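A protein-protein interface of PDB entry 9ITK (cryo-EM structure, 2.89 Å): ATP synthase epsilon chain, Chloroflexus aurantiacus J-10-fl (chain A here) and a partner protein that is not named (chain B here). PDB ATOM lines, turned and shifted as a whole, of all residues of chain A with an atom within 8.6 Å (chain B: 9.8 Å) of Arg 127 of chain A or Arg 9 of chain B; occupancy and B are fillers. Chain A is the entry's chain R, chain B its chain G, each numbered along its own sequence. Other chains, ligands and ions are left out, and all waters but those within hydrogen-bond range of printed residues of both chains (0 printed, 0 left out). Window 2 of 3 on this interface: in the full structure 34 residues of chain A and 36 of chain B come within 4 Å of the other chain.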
ATOM      1  N   ARG A 120      19.782  28.304   3.968  1.00  0.00           N
ATOM      2  CA  ARG A 120      18.335  28.277   3.802  1.00  0.00           C
ATOM      3  C   ARG A 120      17.785  26.863   3.902  1.00  0.00           C
ATOM      4  O   ARG A 120      16.641  26.672   4.327  1.00  0.00           O
ATOM      5  CB  ARG A 120      17.952  28.912   2.467  1.00  0.00           C
ATOM      6  CG  ARG A 120      18.480  30.322   2.288  1.00  0.00           C
ATOM      7  CD  ARG A 120      17.402  31.248   1.754  1.00  0.00           C
ATOM      8  NE  ARG A 120      16.991  30.880   0.405  1.00  0.00           N
ATOM      9  CZ  ARG A 120      17.664  31.192  -0.694  1.00  0.00           C
ATOM     10  NH1 ARG A 120      18.790  31.885  -0.643  1.00  0.00           N
ATOM     11  NH2 ARG A 120      17.194  30.800  -1.875  1.00  0.00           N
ATOM     12  N   LYS A 121      18.577  25.863   3.518  1.00  0.00           N
ATOM     13  CA  LYS A 121      18.141  24.483   3.687  1.00  0.00           C
ATOM     14  C   LYS A 121      18.192  24.057   5.149  1.00  0.00           C
ATOM     15  O   LYS A 121      17.245  23.446   5.652  1.00  0.00           O
ATOM     16  CB  LYS A 121      18.994  23.560   2.825  1.00  0.00           C
ATOM     17  CG  LYS A 121      18.725  22.099   3.023  1.00  0.00           C
ATOM     18  CD  LYS A 121      19.661  21.285   2.168  1.00  0.00           C
ATOM     19  CE  LYS A 121      19.108  19.904   1.945  1.00  0.00           C
ATOM     20  NZ  LYS A 121      19.535  19.033   3.063  1.00  0.00           N
ATOM     21  N   GLU A 122      19.282  24.377   5.851  1.00  0.00           N
ATOM     22  CA  GLU A 122      19.407  23.960   7.246  1.00  0.00           C
ATOM     23  C   GLU A 122      18.329  24.601   8.110  1.00  0.00           C
ATOM     24  O   GLU A 122      17.733  23.942   8.969  1.00  0.00           O
ATOM     25  CB  GLU A 122      20.794  24.310   7.783  1.00  0.00           C
ATOM     26  CG  GLU A 122      21.847  23.239   7.559  1.00  0.00           C
ATOM     27  CD  GLU A 122      23.175  23.591   8.203  1.00  0.00           C
ATOM     28  OE1 GLU A 122      23.426  24.793   8.436  1.00  0.00           O
ATOM     29  OE2 GLU A 122      23.972  22.669   8.471  1.00  0.00           O
ATOM     30  N   MET A 123      18.067  25.893   7.900  1.00  0.00           N
ATOM     31  CA  MET A 123      17.101  26.588   8.743  1.00  0.00           C
ATOM     32  C   MET A 123      15.696  26.033   8.548  1.00  0.00           C
ATOM     33  O   MET A 123      14.914  25.967   9.503  1.00  0.00           O
ATOM     34  CB  MET A 123      17.135  28.092   8.466  1.00  0.00           C
ATOM     35  CG  MET A 123      16.697  28.496   7.071  1.00  0.00           C
ATOM     36  SD  MET A 123      16.743  30.280   6.821  1.00  0.00           S
ATOM     37  CE  MET A 123      15.344  30.796   7.813  1.00  0.00           C
ATOM     38  N   VAL A 124      15.356  25.623   7.324  1.00  0.00           N
ATOM     39  CA  VAL A 124      14.034  25.057   7.092  1.00  0.00           C
ATOM     40  C   VAL A 124      14.004  23.584   7.475  1.00  0.00           C
ATOM     41  O   VAL A 124      12.923  22.995   7.587  1.00  0.00           O
ATOM     42  CB  VAL A 124      13.604  25.264   5.624  1.00  0.00           C
ATOM     43  CG1 VAL A 124      14.429  24.400   4.693  1.00  0.00           C
ATOM     44  CG2 VAL A 124      12.113  25.012   5.443  1.00  0.00           C
ATOM     45  N   ARG A 125      15.168  22.970   7.693  1.00  0.00           N
ATOM     46  CA  ARG A 125      15.188  21.572   8.103  1.00  0.00           C
ATOM     47  C   ARG A 125      14.610  21.371   9.495  1.00  0.00           C
ATOM     48  O   ARG A 125      13.904  20.385   9.730  1.00  0.00           O
ATOM     49  CB  ARG A 125      16.610  21.014   8.059  1.00  0.00           C
ATOM     50  CG  ARG A 125      17.114  20.600   6.680  1.00  0.00           C
ATOM     51  CD  ARG A 125      16.034  20.079   5.741  1.00  0.00           C
ATOM     52  NE  ARG A 125      15.150  19.101   6.361  1.00  0.00           N
ATOM     53  CZ  ARG A 125      15.396  17.803   6.407  1.00  0.00           C
ATOM     54  NH1 ARG A 125      16.534  17.302   5.959  1.00  0.00           N
ATOM     55  NH2 ARG A 125      14.488  16.989   6.939  1.00  0.00           N
ATOM     56  N   LEU A 126      14.912  22.265  10.436  1.00  0.00           N
ATOM     57  CA  LEU A 126      14.295  22.164  11.752  1.00  0.00           C
ATOM     58  C   LEU A 126      12.850  22.639  11.730  1.00  0.00           C
ATOM     59  O   LEU A 126      12.027  22.142  12.506  1.00  0.00           O
ATOM     60  CB  LEU A 126      15.108  22.956  12.780  1.00  0.00           C
ATOM     61  CG  LEU A 126      14.730  22.795  14.258  1.00  0.00           C
ATOM     62  CD1 LEU A 126      15.971  22.847  15.134  1.00  0.00           C
ATOM     63  CD2 LEU A 126      13.737  23.863  14.700  1.00  0.00           C
ATOM     64  N   ARG A 127      12.521  23.584  10.848  1.00  0.00           N
ATOM     65  CA  ARG A 127      11.159  24.093  10.774  1.00  0.00           C
ATOM     66  C   ARG A 127      10.171  23.043  10.285  1.00  0.00           C
ATOM     67  O   ARG A 127       8.985  23.125  10.621  1.00  0.00           O
ATOM     68  CB  ARG A 127      11.103  25.319   9.865  1.00  0.00           C
ATOM     69  CG  ARG A 127      11.846  26.523  10.409  1.00  0.00           C
ATOM     70  CD  ARG A 127      11.422  27.786   9.689  1.00  0.00           C
ATOM     71  NE  ARG A 127      11.284  27.565   8.254  1.00  0.00           N
ATOM     72  CZ  ARG A 127      10.826  28.468   7.399  1.00  0.00           C
ATOM     73  NH1 ARG A 127      10.448  29.671   7.800  1.00  0.00           N
ATOM     74  NH2 ARG A 127      10.744  28.156   6.109  1.00  0.00           N
ATOM     75  N   VAL A 128      10.625  22.063   9.505  1.00  0.00           N
ATOM     76  CA  VAL A 128       9.759  20.986   9.043  1.00  0.00           C
ATOM     77  C   VAL A 128       9.666  19.867  10.075  1.00  0.00           C
ATOM     78  O   VAL A 128       8.772  19.020   9.992  1.00  0.00           O
ATOM     79  CB  VAL A 128      10.230  20.450   7.679  1.00  0.00           C
ATOM     80  CG1 VAL A 128      11.539  19.698   7.815  1.00  0.00           C
ATOM     81  CG2 VAL A 128       9.166  19.588   7.021  1.00  0.00           C
ATOM     82  N   ALA A 129      10.549  19.865  11.067  1.00  0.00           N
ATOM     83  CA  ALA A 129      10.521  18.863  12.123  1.00  0.00           C
ATOM     84  C   ALA A 129       9.477  19.216  13.175  1.00  0.00           C
ATOM     85  O   ALA A 129       9.763  19.206  14.372  1.00  0.00           O
ATOM     86  CB  ALA A 129      11.893  18.728  12.764  1.00  0.00           C
ATOM     87  N   PRO B   2      -1.742  17.576  11.725  1.00  0.00           N
ATOM     88  CA  PRO B   2      -2.818  16.956  10.947  1.00  0.00           C
ATOM     89  C   PRO B   2      -4.136  17.703  11.088  1.00  0.00           C
ATOM     90  O   PRO B   2      -5.152  17.099  11.421  1.00  0.00           O
ATOM     91  CB  PRO B   2      -2.925  15.555  11.552  1.00  0.00           C
ATOM     92  CG  PRO B   2      -1.583  15.299  12.138  1.00  0.00           C
ATOM     93  CD  PRO B   2      -1.123  16.623  12.660  1.00  0.00           C
ATOM     94  N   SER B   3      -4.111  19.011  10.834  1.00  0.00           N
ATOM     95  CA  SER B   3      -5.296  19.850  10.955  1.00  0.00           C
ATOM     96  C   SER B   3      -5.610  20.591   9.662  1.00  0.00           C
ATOM     97  O   SER B   3      -6.277  21.628   9.697  1.00  0.00           O
ATOM     98  CB  SER B   3      -5.132  20.842  12.105  1.00  0.00           C
ATOM     99  OG  SER B   3      -4.222  21.870  11.759  1.00  0.00           O
ATOM    100  N   SER B   4      -5.119  20.094   8.526  1.00  0.00           N
ATOM    101  CA  SER B   4      -5.325  20.648   7.190  1.00  0.00           C
ATOM    102  C   SER B   4      -4.661  22.003   7.009  1.00  0.00           C
ATOM    103  O   SER B   4      -4.699  22.551   5.904  1.00  0.00           O
ATOM    104  CB  SER B   4      -6.809  20.777   6.823  1.00  0.00           C
ATOM    105  OG  SER B   4      -6.975  21.604   5.687  1.00  0.00           O
ATOM    106  N   ARG B   5      -4.062  22.562   8.049  1.00  0.00           N
ATOM    107  CA  ARG B   5      -3.290  23.793   7.969  1.00  0.00           C
ATOM    108  C   ARG B   5      -1.853  23.596   8.408  1.00  0.00           C
ATOM    109  O   ARG B   5      -0.953  24.245   7.871  1.00  0.00           O
ATOM    110  CB  ARG B   5      -3.946  24.887   8.822  1.00  0.00           C
ATOM    111  CG  ARG B   5      -3.304  26.253   8.682  1.00  0.00           C
ATOM    112  CD  ARG B   5      -4.037  27.290   9.514  1.00  0.00           C
ATOM    113  NE  ARG B   5      -4.082  26.920  10.922  1.00  0.00           N
ATOM    114  CZ  ARG B   5      -3.205  27.325  11.830  1.00  0.00           C
ATOM    115  NH1 ARG B   5      -2.199  28.121  11.510  1.00  0.00           N
ATOM    116  NH2 ARG B   5      -3.341  26.919  13.088  1.00  0.00           N
ATOM    117  N   GLU B   6      -1.615  22.714   9.379  1.00  0.00           N
ATOM    118  CA  GLU B   6      -0.249  22.329   9.705  1.00  0.00           C
ATOM    119  C   GLU B   6       0.385  21.559   8.556  1.00  0.00           C
ATOM    120  O   GLU B   6       1.578  21.719   8.277  1.00  0.00           O
ATOM    121  CB  GLU B   6      -0.231  21.499  10.986  1.00  0.00           C
ATOM    122  CG  GLU B   6       1.117  21.466  11.686  1.00  0.00           C
ATOM    123  CD  GLU B   6       2.024  20.371  11.163  1.00  0.00           C
ATOM    124  OE1 GLU B   6       1.503  19.384  10.603  1.00  0.00           O
ATOM    125  OE2 GLU B   6       3.258  20.497  11.313  1.00  0.00           O
ATOM    126  N   ILE B   7      -0.398  20.715   7.879  1.00  0.00           N
ATOM    127  CA  ILE B   7       0.125  19.967   6.743  1.00  0.00           C
ATOM    128  C   ILE B   7       0.467  20.901   5.593  1.00  0.00           C
ATOM    129  O   ILE B   7       1.425  20.656   4.851  1.00  0.00           O
ATOM    130  CB  ILE B   7      -0.870  18.879   6.309  1.00  0.00           C
ATOM    131  CG1 ILE B   7      -1.384  18.122   7.530  1.00  0.00           C
ATOM    132  CG2 ILE B   7      -0.207  17.917   5.353  1.00  0.00           C
ATOM    133  CD1 ILE B   7      -2.268  16.951   7.187  1.00  0.00           C
ATOM    134  N   LYS B   8      -0.305  21.973   5.409  1.00  0.00           N
ATOM    135  CA  LYS B   8       0.052  22.967   4.403  1.00  0.00           C
ATOM    136  C   LYS B   8       1.409  23.585   4.707  1.00  0.00           C
ATOM    137  O   LYS B   8       2.189  23.869   3.793  1.00  0.00           O
ATOM    138  CB  LYS B   8      -1.021  24.049   4.320  1.00  0.00           C
ATOM    139  CG  LYS B   8      -2.188  23.696   3.422  1.00  0.00           C
ATOM    140  CD  LYS B   8      -1.709  23.182   2.078  1.00  0.00           C
ATOM    141  CE  LYS B   8      -1.297  24.321   1.163  1.00  0.00           C
ATOM    142  NZ  LYS B   8      -1.133  23.862  -0.243  1.00  0.00           N
ATOM    143  N   ARG B   9       1.701  23.813   5.988  1.00  0.00           N
ATOM    144  CA  ARG B   9       3.020  24.305   6.364  1.00  0.00           C
ATOM    145  C   ARG B   9       4.101  23.280   6.046  1.00  0.00           C
ATOM    146  O   ARG B   9       5.173  23.635   5.544  1.00  0.00           O
ATOM    147  CB  ARG B   9       3.040  24.662   7.849  1.00  0.00           C
ATOM    148  CG  ARG B   9       4.084  25.698   8.223  1.00  0.00           C
ATOM    149  CD  ARG B   9       4.285  25.744   9.726  1.00  0.00           C
ATOM    150  NE  ARG B   9       4.291  24.410  10.309  1.00  0.00           N
ATOM    151  CZ  ARG B   9       5.388  23.741  10.638  1.00  0.00           C
ATOM    152  NH1 ARG B   9       6.592  24.258  10.457  1.00  0.00           N
ATOM    153  NH2 ARG B   9       5.275  22.523  11.162  1.00  0.00           N
ATOM    154  N   ARG B  10       3.839  22.003   6.334  1.00  0.00           N
ATOM    155  CA  ARG B  10       4.819  20.962   6.037  1.00  0.00           C
ATOM    156  C   ARG B  10       5.065  20.854   4.539  1.00  0.00           C
ATOM    157  O   ARG B  10       6.208  20.712   4.095  1.00  0.00           O
ATOM    158  CB  ARG B  10       4.354  19.621   6.604  1.00  0.00           C
ATOM    159  CG  ARG B  10       4.398  19.539   8.117  1.00  0.00           C
ATOM    160  CD  ARG B  10       5.637  18.809   8.609  1.00  0.00           C
ATOM    161  NE  ARG B  10       5.452  17.363   8.639  1.00  0.00           N
ATOM    162  CZ  ARG B  10       6.369  16.479   8.269  1.00  0.00           C
ATOM    163  NH1 ARG B  10       7.559  16.858   7.836  1.00  0.00           N
ATOM    164  NH2 ARG B  10       6.088  15.180   8.345  1.00  0.00           N
ATOM    165  N   ILE B  11       3.999  20.924   3.740  1.00  0.00           N
ATOM    166  CA  ILE B  11       4.151  20.840   2.291  1.00  0.00           C
ATOM    167  C   ILE B  11       4.968  22.014   1.772  1.00  0.00           C
ATOM    168  O   ILE B  11       5.832  21.853   0.903  1.00  0.00           O
ATOM    169  CB  ILE B  11       2.773  20.766   1.611  1.00  0.00           C
ATOM    170  CG1 ILE B  11       2.112  19.421   1.901  1.00  0.00           C
ATOM    171  CG2 ILE B  11       2.903  20.974   0.117  1.00  0.00           C
ATOM    172  CD1 ILE B  11       0.748  19.274   1.285  1.00  0.00           C
ATOM    173  N   ARG B  12       4.708  23.213   2.293  1.00  0.00           N
ATOM    174  CA  ARG B  12       5.477  24.380   1.878  1.00  0.00           C
ATOM    175  C   ARG B  12       6.948  24.230   2.240  1.00  0.00           C
ATOM    176  O   ARG B  12       7.829  24.583   1.448  1.00  0.00           O
ATOM    177  CB  ARG B  12       4.900  25.642   2.514  1.00  0.00           C
ATOM    178  CG  ARG B  12       5.579  26.924   2.062  1.00  0.00           C
ATOM    179  CD  ARG B  12       5.444  27.144   0.553  1.00  0.00           C
ATOM    180  NE  ARG B  12       4.137  26.815  -0.013  1.00  0.00           N
ATOM    181  CZ  ARG B  12       2.962  27.247   0.434  1.00  0.00           C
ATOM    182  NH1 ARG B  12       2.869  28.118   1.426  1.00  0.00           N
ATOM    183  NH2 ARG B  12       1.848  26.808  -0.146  1.00  0.00           N
ATOM    184  N   SER B  13       7.235  23.712   3.436  1.00  0.00           N
ATOM    185  CA  SER B  13       8.621  23.563   3.863  1.00  0.00           C
ATOM    186  C   SER B  13       9.362  22.559   2.989  1.00  0.00           C
ATOM    187  O   SER B  13      10.478  22.825   2.531  1.00  0.00           O
ATOM    188  CB  SER B  13       8.675  23.142   5.331  1.00  0.00           C
ATOM    189  OG  SER B  13       8.246  24.193   6.176  1.00  0.00           O
ATOM    190  N   VAL B  14       8.752  21.399   2.740  1.00  0.00           N
ATOM    191  CA  VAL B  14       9.415  20.382   1.930  1.00  0.00           C
ATOM    192  C   VAL B  14       9.569  20.862   0.493  1.00  0.00           C
ATOM    193  O   VAL B  14      10.573  20.569  -0.167  1.00  0.00           O
ATOM    194  CB  VAL B  14       8.653  19.049   2.008  1.00  0.00           C
ATOM    195  CG1 VAL B  14       9.397  17.975   1.248  1.00  0.00           C
ATOM    196  CG2 VAL B  14       8.484  18.630   3.451  1.00  0.00           C
ATOM    197  N   LYS B  15       8.588  21.608  -0.017  1.00  0.00           N
ATOM    198  CA  LYS B  15       8.712  22.155  -1.363  1.00  0.00           C
ATOM    199  C   LYS B  15       9.880  23.123  -1.466  1.00  0.00           C
ATOM    200  O   LYS B  15      10.543  23.186  -2.507  1.00  0.00           O
ATOM    201  CB  LYS B  15       7.415  22.843  -1.779  1.00  0.00           C
ATOM    202  CG  LYS B  15       6.474  21.954  -2.568  1.00  0.00           C
ATOM    203  CD  LYS B  15       5.215  22.700  -2.965  1.00  0.00           C
ATOM    204  CE  LYS B  15       4.368  21.877  -3.916  1.00  0.00           C
ATOM    205  NZ  LYS B  15       3.010  22.458  -4.085  1.00  0.00           N
ATOM    206  N   ASN B  16      10.143  23.894  -0.409  1.00  0.00           N
ATOM    207  CA  ASN B  16      11.328  24.746  -0.394  1.00  0.00           C
ATOM    208  C   ASN B  16      12.598  23.908  -0.423  1.00  0.00           C
ATOM    209  O   ASN B  16      13.567  24.250  -1.111  1.00  0.00           O
ATOM    210  CB  ASN B  16      11.310  25.656   0.832  1.00  0.00           C
ATOM    211  CG  ASN B  16      10.291  26.766   0.716  1.00  0.00           C
ATOM    212  OD1 ASN B  16       9.679  26.951  -0.335  1.00  0.00           O
ATOM    213  ND2 ASN B  16      10.104  27.514   1.795  1.00  0.00           N
ATOM    214  N   VAL B  17      12.614  22.805   0.325  1.00  0.00           N
ATOM    215  CA  VAL B  17      13.768  21.915   0.308  1.00  0.00           C
ATOM    216  C   VAL B  17      13.958  21.318  -1.079  1.00  0.00           C
ATOM    217  O   VAL B  17      15.081  21.241  -1.587  1.00  0.00           O
ATOM    218  CB  VAL B  17      13.617  20.822   1.380  1.00  0.00           C
ATOM    219  CG1 VAL B  17      14.784  19.862   1.321  1.00  0.00           C
ATOM    220  CG2 VAL B  17      13.514  21.446   2.754  1.00  0.00           C
ATOM    221  N   ILE B  20      15.532  23.961  -3.275  1.00  0.00           N
ATOM    222  CA  ILE B  20      16.931  24.210  -2.939  1.00  0.00           C
ATOM    223  C   ILE B  20      17.793  23.019  -3.330  1.00  0.00           C
ATOM    224  O   ILE B  20      18.861  23.175  -3.932  1.00  0.00           O
ATOM    225  CB  ILE B  20      17.071  24.540  -1.444  1.00  0.00           C
ATOM    226  CG1 ILE B  20      16.420  25.888  -1.136  1.00  0.00           C
ATOM    227  CG2 ILE B  20      18.532  24.546  -1.036  1.00  0.00           C
ATOM    228  CD1 ILE B  20      16.729  26.409   0.241  1.00  0.00           C
ATOM    229  N   VAL B 259       6.406  15.181  -0.564  1.00  0.00           N
ATOM    230  CA  VAL B 259       5.351  16.137  -0.890  1.00  0.00           C
ATOM    231  C   VAL B 259       4.114  15.410  -1.396  1.00  0.00           C
ATOM    232  O   VAL B 259       2.984  15.736  -1.013  1.00  0.00           O
ATOM    233  CB  VAL B 259       5.856  17.170  -1.914  1.00  0.00           C
ATOM    234  CG1 VAL B 259       4.700  17.983  -2.458  1.00  0.00           C
ATOM    235  CG2 VAL B 259       6.875  18.082  -1.276  1.00  0.00           C
ATOM    236  N   LEU B 262       2.564  13.878   1.614  1.00  0.00           N
ATOM    237  CA  LEU B 262       1.931  14.912   2.427  1.00  0.00           C
ATOM    238  C   LEU B 262       0.691  15.473   1.747  1.00  0.00           C
ATOM    239  O   LEU B 262      -0.328  15.714   2.405  1.00  0.00           O
ATOM    240  CB  LEU B 262       2.925  16.030   2.729  1.00  0.00           C
ATOM    241  CG  LEU B 262       3.937  15.756   3.838  1.00  0.00           C
ATOM    242  CD1 LEU B 262       4.891  16.926   3.972  1.00  0.00           C
ATOM    243  CD2 LEU B 262       3.225  15.489   5.150  1.00  0.00           C
ATOM    244  N   PHE B 266      -2.800  15.624   3.248  1.00  0.00           N
ATOM    245  CA  PHE B 266      -3.488  16.902   3.394  1.00  0.00           C
ATOM    246  C   PHE B 266      -4.884  16.842   2.798  1.00  0.00           C
ATOM    247  O   PHE B 266      -5.831  17.414   3.350  1.00  0.00           O
ATOM    248  CB  PHE B 266      -2.681  18.015   2.733  1.00  0.00           C
ATOM    249  CG  PHE B 266      -3.504  19.200   2.324  1.00  0.00           C
ATOM    250  CD1 PHE B 266      -3.953  20.104   3.265  1.00  0.00           C
ATOM    251  CD2 PHE B 266      -3.825  19.412   0.997  1.00  0.00           C
ATOM    252  CE1 PHE B 266      -4.706  21.196   2.893  1.00  0.00           C
ATOM    253  CE2 PHE B 266      -4.579  20.502   0.620  1.00  0.00           C
ATOM    254  CZ  PHE B 266      -5.020  21.394   1.570  1.00  0.00           C
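NH1 of Arg 9 of chain B sits at hydrogen-bond distance from O of Arg 127 of chain A, 2.7 Å away.
The guanidinium group (NH1) of Arg 10 of chain B sits close to the backbone carbonyl oxygen (O) of Val 128 of chain A (3.3 Å).
OE2 of Glu 6 of chain B is in salt-bridge range of NH2 of Arg 9 of chain B.
O of Arg 9 of chain B sits at hydrogen-bond distance from OG of Ser 13 of chain B (3.2 Å).
Ile 20 of chain B touches Arg 120 of chain A (CD1 to CB, 3.6 Å).
Ile 20 of chain B touches Lys 121 of chain A (CD1 to N, 3.8 Å).
CB of Ser 13 of chain B touches CG2 of Val 124 of chain A (3.9 Å).
CG2 of Val 17 of chain B touches CG1 of Val 124 of chain A, at 3.7 Å.
Val 128 of chain A touches Ser 13 of chain B.
Val 14 of chain B touches Val 128 of chain A (CG2 to CG2, 3.8 Å).
Arg 127 of chain A touches just one residue of chain B: Arg 9.
Of chain A, only Arg 127 (2.7 Å) comes within 4 Å of Arg 9 of chain B.
No residue of chain B comes within 4 Å of Ala 129 of chain A.
Of the printed residues of chain A, Ile 20 of chain B touches Arg 120 (3.6 Å) and Lys 121 (3.8 Å).
Printed residues of chain A within 4 Å of Val 17 of chain B: Val 124 (3.7 Å).
Printed residues of chain A within 4 Å of Ser 13 of chain B: Val 124 and Val 128.
Of the printed residues of chain B, Lys 121 of chain A touches Ile 20 (3.8 Å).
Ile 7 of chain B touches none of the printed residues of chain A.
Val 259 of chain B touches none of the printed residues of chain A.
The nearest residue of chain A that does not touch Arg 9 of chain B is Val 128 of chain A (4.7 Å).
Among the printed residues, no Asp or Glu carboxylate lies within 4 Å of a Lys or Arg side-chain nitrogen of the other chain.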
